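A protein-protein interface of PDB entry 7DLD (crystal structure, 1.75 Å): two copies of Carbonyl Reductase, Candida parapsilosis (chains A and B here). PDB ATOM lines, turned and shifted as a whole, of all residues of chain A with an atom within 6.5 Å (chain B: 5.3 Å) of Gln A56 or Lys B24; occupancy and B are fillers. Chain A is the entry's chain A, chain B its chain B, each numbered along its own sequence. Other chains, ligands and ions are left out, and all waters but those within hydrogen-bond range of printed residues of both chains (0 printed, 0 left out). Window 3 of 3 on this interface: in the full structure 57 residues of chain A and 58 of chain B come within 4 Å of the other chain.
The side-chain amide nitrogen of Gln A56 is in hydrogen-bond range of the backbone carbonyl oxygen of Lys B24 (3.1 Å).
OE1 of Gln A56 is in hydrogen-bond range of N of Val B26, at 2.8 Å.
The side-chain amide nitrogen (NE2) of Gln A248 lies within hydrogen-bond range of the backbone carbonyl oxygen (O) of Ser B23.
Gln A56 touches just these residues of chain B: Lys B24, Asn B25, Val B26 and Leu B27.
Lys B24 touches just these residues of chain A: Gln A56 (3.1 Å) and Gln A248 (3.9 Å).
Of the printed residues of chain B, Val A251 touches Val B26 (3.8 Å).
Printed residues of chain B within 4 Å of Ala A53: Val B26 (3.4 Å).
Printed residues of chain B within 4 Å of Gln A248: Ser B23 (3.4 Å) and Lys B24 (3.9 Å).
Printed residues of chain A within 4 Å of Val B26: Ala A53 (3.4 Å), Gln A56 (2.8 Å) and Val A251 (3.8 Å).
Ala A51 touches none of the printed residues of chain B.
Glu A52 touches none of the printed residues of chain B.
The nearest printed residue of chain B that does not touch Gln A56 is Ser B23 (6.5 Å).
The side-chain hydroxyl (OH) of Tyr A81 lies within hydrogen-bond range of the side-chain amide nitrogen (NE2) of Gln A56, at 3.2 Å.
N of Leu B27 is in hydrogen-bond range of OD1 of Asn B25 (3.0 Å).
No position is printed for both chains.
Of the 8 pairs that touch across the chains among the printed residues, none has its exchanged pair printed and touching as well.
Among the printed residues, pairs that only touch across the chains: Ala A53 with Val B26 (3.4 Å), Gln A56 with Asn B25 (3.4 Å), Gln A56 with Leu B27 (3.7 Å), Gln A248 with Lys B24 (3.9 Å) and Val A251 with Val B26 (3.8 Å).
Of the 6 printed residues of chain B, 5 touch a printed residue of chain A.
Hydrophobic or aromatic side chains of chain B that line the printed part of chain A: Val B26 and Leu B27.
Of the 13 printed residues of chain A, 4 touch a printed residue of chain B.
Printed residues of chain A that touch a printed residue of chain B: Ala A53, Gln A56, Gln A248 and Val A251.
Hydrophobic or aromatic side chains of chain A within 4 Å of the printed part of chain B: Ala A53 and Val A251.
Among the printed residues, 8 pairs touch across the chains.
Among the printed residues, no Asp or Glu carboxylate lies within 4 Å of a Lys or Arg side-chain nitrogen of the other chain.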
ATOM      1  N   ALA A  49       5.260  -1.568  -7.804  1.00  0.00           N
ATOM      2  CA  ALA A  49       4.021  -2.330  -7.910  1.00  0.00           C
ATOM      3  C   ALA A  49       4.286  -3.763  -8.377  1.00  0.00           C
ATOM      4  O   ALA A  49       3.610  -4.700  -7.937  1.00  0.00           O
ATOM      5  CB  ALA A  49       3.047  -1.611  -8.853  1.00  0.00           C
ATOM      6  N   ALA A  51       7.221  -5.464  -7.973  1.00  0.00           N
ATOM      7  CA  ALA A  51       7.892  -6.124  -6.855  1.00  0.00           C
ATOM      8  C   ALA A  51       6.897  -6.601  -5.801  1.00  0.00           C
ATOM      9  O   ALA A  51       7.012  -7.723  -5.291  1.00  0.00           O
ATOM     10  CB  ALA A  51       8.915  -5.176  -6.229  1.00  0.00           C
ATOM     11  N   GLU A  52       5.908  -5.765  -5.470  1.00  0.00           N
ATOM     12  CA  GLU A  52       4.933  -6.145  -4.454  1.00  0.00           C
ATOM     13  C   GLU A  52       4.000  -7.243  -4.954  1.00  0.00           C
ATOM     14  O   GLU A  52       3.644  -8.149  -4.195  1.00  0.00           O
ATOM     15  CB  GLU A  52       4.134  -4.916  -3.997  1.00  0.00           C
ATOM     16  CG  GLU A  52       2.944  -5.247  -3.105  1.00  0.00           C
ATOM     17  CD  GLU A  52       2.633  -4.156  -2.083  1.00  0.00           C
ATOM     18  OE1 GLU A  52       2.116  -4.500  -0.997  1.00  0.00           O
ATOM     19  OE2 GLU A  52       2.906  -2.966  -2.360  1.00  0.00           O
ATOM     20  N   ALA A  53       3.599  -7.189  -6.229  1.00  0.00           N
ATOM     21  CA  ALA A  53       2.746  -8.241  -6.785  1.00  0.00           C
ATOM     22  C   ALA A  53       3.469  -9.586  -6.838  1.00  0.00           C
ATOM     23  O   ALA A  53       2.856 -10.645  -6.645  1.00  0.00           O
ATOM     24  CB  ALA A  53       2.268  -7.840  -8.184  1.00  0.00           C
ATOM     25  N   TYR A  54       4.767  -9.569  -7.125  1.00  0.00           N
ATOM     26  CA  TYR A  54       5.526 -10.813  -7.156  1.00  0.00           C
ATOM     27  C   TYR A  54       5.635 -11.421  -5.762  1.00  0.00           C
ATOM     28  O   TYR A  54       5.558 -12.644  -5.604  1.00  0.00           O
ATOM     29  CB  TYR A  54       6.902 -10.550  -7.750  1.00  0.00           C
ATOM     30  CG  TYR A  54       6.901 -10.386  -9.264  1.00  0.00           C
ATOM     31  CD1 TYR A  54       8.051  -9.993  -9.925  1.00  0.00           C
ATOM     32  CD2 TYR A  54       5.753 -10.615 -10.020  1.00  0.00           C
ATOM     33  CE1 TYR A  54       8.083  -9.845 -11.305  1.00  0.00           C
ATOM     34  CE2 TYR A  54       5.775 -10.470 -11.442  1.00  0.00           C
ATOM     35  CZ  TYR A  54       6.949 -10.064 -12.059  1.00  0.00           C
ATOM     36  OH  TYR A  54       7.045  -9.900 -13.438  1.00  0.00           O
ATOM     37  N   ALA A  55       5.782 -10.575  -4.742  1.00  0.00           N
ATOM     38  CA  ALA A  55       5.764 -11.054  -3.363  1.00  0.00           C
ATOM     39  C   ALA A  55       4.415 -11.678  -3.020  1.00  0.00           C
ATOM     40  O   ALA A  55       4.349 -12.753  -2.413  1.00  0.00           O
ATOM     41  CB  ALA A  55       6.087  -9.897  -2.418  1.00  0.00           C
ATOM     42  N   GLN A  56       3.325 -11.008  -3.400  1.00  0.00           N
ATOM     43  CA  GLN A  56       1.991 -11.586  -3.262  1.00  0.00           C
ATOM     44  C   GLN A  56       1.891 -12.952  -3.934  1.00  0.00           C
ATOM     45  O   GLN A  56       1.221 -13.857  -3.425  1.00  0.00           O
ATOM     46  CB  GLN A  56       0.958 -10.626  -3.849  1.00  0.00           C
ATOM     47  CG  GLN A  56       0.883  -9.309  -3.092  1.00  0.00           C
ATOM     48  CD  GLN A  56       0.007  -8.262  -3.770  1.00  0.00           C
ATOM     49  OE1 GLN A  56      -0.481  -8.461  -4.883  1.00  0.00           O
ATOM     50  NE2 GLN A  56      -0.201  -7.141  -3.087  1.00  0.00           N
ATOM     51  N   ALA A  57       2.543 -13.120  -5.083  1.00  0.00           N
ATOM     52  CA  ALA A  57       2.539 -14.404  -5.770  1.00  0.00           C
ATOM     53  C   ALA A  57       3.493 -15.412  -5.144  1.00  0.00           C
ATOM     54  O   ALA A  57       3.547 -16.558  -5.604  1.00  0.00           O
ATOM     55  CB  ALA A  57       2.884 -14.209  -7.248  1.00  0.00           C
ATOM     56  N   GLY A  58       4.248 -15.016  -4.125  1.00  0.00           N
ATOM     57  CA  GLY A  58       5.073 -15.935  -3.374  1.00  0.00           C
ATOM     58  C   GLY A  58       6.559 -15.866  -3.642  1.00  0.00           C
ATOM     59  O   GLY A  58       7.303 -16.682  -3.092  1.00  0.00           O
ATOM     60  N   ALA A  59       7.022 -14.919  -4.447  1.00  0.00           N
ATOM     61  CA  ALA A  59       8.419 -14.874  -4.851  1.00  0.00           C
ATOM     62  C   ALA A  59       9.268 -14.064  -3.879  1.00  0.00           C
ATOM     63  O   ALA A  59       8.824 -13.040  -3.348  1.00  0.00           O
ATOM     64  CB  ALA A  59       8.546 -14.274  -6.250  1.00  0.00           C
ATOM     65  N   TYR A  81       4.571 -10.174   3.616  1.00  0.00           N
ATOM     66  CA  TYR A  81       4.212 -11.385   2.895  1.00  0.00           C
ATOM     67  C   TYR A  81       5.022 -12.604   3.309  1.00  0.00           C
ATOM     68  O   TYR A  81       4.743 -13.706   2.823  1.00  0.00           O
ATOM     69  CB  TYR A  81       4.346 -11.148   1.382  1.00  0.00           C
ATOM     70  CG  TYR A  81       3.513  -9.974   0.930  1.00  0.00           C
ATOM     71  CD1 TYR A  81       4.074  -8.713   0.785  1.00  0.00           C
ATOM     72  CD2 TYR A  81       2.151 -10.116   0.699  1.00  0.00           C
ATOM     73  CE1 TYR A  81       3.303  -7.624   0.390  1.00  0.00           C
ATOM     74  CE2 TYR A  81       1.375  -9.042   0.316  1.00  0.00           C
ATOM     75  CZ  TYR A  81       1.954  -7.800   0.157  1.00  0.00           C
ATOM     76  OH  TYR A  81       1.174  -6.742  -0.222  1.00  0.00           O
ATOM     77  N   GLN A 248      -1.746  -0.680 -10.874  1.00  0.00           N
ATOM     78  CA  GLN A 248      -2.342  -1.957 -10.505  1.00  0.00           C
ATOM     79  C   GLN A 248      -2.964  -2.674 -11.698  1.00  0.00           C
ATOM     80  O   GLN A 248      -3.265  -3.867 -11.607  1.00  0.00           O
ATOM     81  CB  GLN A 248      -3.378  -1.742  -9.398  1.00  0.00           C
ATOM     82  CG  GLN A 248      -3.929  -3.024  -8.770  1.00  0.00           C
ATOM     83  CD  GLN A 248      -2.866  -3.855  -8.056  1.00  0.00           C
ATOM     84  OE1 GLN A 248      -1.756  -3.384  -7.795  1.00  0.00           O
ATOM     85  NE2 GLN A 248      -3.209  -5.100  -7.733  1.00  0.00           N
ATOM     86  N   VAL A 251       0.049  -5.127 -13.147  1.00  0.00           N
ATOM     87  CA  VAL A 251       0.741  -6.205 -12.442  1.00  0.00           C
ATOM     88  C   VAL A 251       0.324  -7.567 -12.965  1.00  0.00           C
ATOM     89  O   VAL A 251       1.119  -8.515 -12.920  1.00  0.00           O
ATOM     90  CB  VAL A 251       0.534  -6.113 -10.918  1.00  0.00           C
ATOM     91  CG1 VAL A 251       1.140  -4.826 -10.385  1.00  0.00           C
ATOM     92  CG2 VAL A 251      -0.942  -6.213 -10.559  1.00  0.00           C
ATOM     93  N   LEU B  22     -10.105  -2.517  -7.791  1.00  0.00           N
ATOM     94  CA  LEU B  22      -9.513  -3.827  -8.031  1.00  0.00           C
ATOM     95  C   LEU B  22      -8.988  -4.421  -6.734  1.00  0.00           C
ATOM     96  O   LEU B  22      -8.607  -3.695  -5.815  1.00  0.00           O
ATOM     97  CB  LEU B  22      -8.352  -3.742  -9.040  1.00  0.00           C
ATOM     98  CG  LEU B  22      -8.632  -3.224 -10.456  1.00  0.00           C
ATOM     99  CD1 LEU B  22      -7.327  -2.845 -11.153  1.00  0.00           C
ATOM    100  CD2 LEU B  22      -9.360  -4.279 -11.272  1.00  0.00           C
ATOM    101  N   SER B  23      -8.913  -5.752  -6.691  1.00  0.00           N
ATOM    102  CA  SER B  23      -8.358  -6.429  -5.526  1.00  0.00           C
ATOM    103  C   SER B  23      -6.948  -5.931  -5.226  1.00  0.00           C
ATOM    104  O   SER B  23      -6.198  -5.529  -6.121  1.00  0.00           O
ATOM    105  CB  SER B  23      -8.329  -7.942  -5.747  1.00  0.00           C
ATOM    106  OG  SER B  23      -9.628  -8.460  -5.966  1.00  0.00           O
ATOM    107  N   LYS B  24      -6.598  -5.954  -3.940  1.00  0.00           N
ATOM    108  CA  LYS B  24      -5.262  -5.561  -3.511  1.00  0.00           C
ATOM    109  C   LYS B  24      -4.229  -6.619  -3.864  1.00  0.00           C
ATOM    110  O   LYS B  24      -3.049  -6.300  -4.047  1.00  0.00           O
ATOM    111  CB  LYS B  24      -5.245  -5.325  -2.000  1.00  0.00           C
ATOM    112  CG  LYS B  24      -4.642  -4.004  -1.574  1.00  0.00           C
ATOM    113  CD  LYS B  24      -5.726  -3.012  -1.180  1.00  0.00           C
ATOM    114  CE  LYS B  24      -5.191  -1.593  -1.172  1.00  0.00           C
ATOM    115  NZ  LYS B  24      -4.642  -1.230  -2.507  1.00  0.00           N
ATOM    116  N   ASN B  25      -4.646  -7.875  -3.948  1.00  0.00           N
ATOM    117  CA  ASN B  25      -3.740  -8.989  -4.176  1.00  0.00           C
ATOM    118  C   ASN B  25      -3.834  -9.447  -5.627  1.00  0.00           C
ATOM    119  O   ASN B  25      -4.924  -9.749  -6.120  1.00  0.00           O
ATOM    120  CB  ASN B  25      -4.061 -10.142  -3.229  1.00  0.00           C
ATOM    121  CG  ASN B  25      -3.040 -11.248  -3.307  1.00  0.00           C
ATOM    122  OD1 ASN B  25      -3.131 -12.132  -4.159  1.00  0.00           O
ATOM    123  ND2 ASN B  25      -2.047 -11.200  -2.423  1.00  0.00           N
ATOM    124  N   VAL B  26      -2.681  -9.517  -6.296  1.00  0.00           N
ATOM    125  CA  VAL B  26      -2.645  -9.788  -7.734  1.00  0.00           C
ATOM    126  C   VAL B  26      -3.346 -11.093  -8.093  1.00  0.00           C
ATOM    127  O   VAL B  26      -3.931 -11.211  -9.176  1.00  0.00           O
ATOM    128  CB  VAL B  26      -1.188  -9.779  -8.235  1.00  0.00           C
ATOM    129  CG1 VAL B  26      -0.369 -10.897  -7.573  1.00  0.00           C
ATOM    130  CG2 VAL B  26      -1.144  -9.893  -9.760  1.00  0.00           C
ATOM    131  N   LEU B  27      -3.312 -12.089  -7.201  1.00  0.00           N
ATOM    132  CA  LEU B  27      -3.892 -13.386  -7.542  1.00  0.00           C
ATOM    133  C   LEU B  27      -5.412 -13.323  -7.617  1.00  0.00           C
ATOM    134  O   LEU B  27      -6.019 -14.041  -8.423  1.00  0.00           O
ATOM    135  CB  LEU B  27      -3.446 -14.445  -6.530  1.00  0.00           C
ATOM    136  CG  LEU B  27      -1.931 -14.616  -6.471  1.00  0.00           C
ATOM    137  CD1 LEU B  27      -1.529 -15.486  -5.289  1.00  0.00           C
ATOM    138  CD2 LEU B  27      -1.423 -15.204  -7.777  1.00  0.00           C
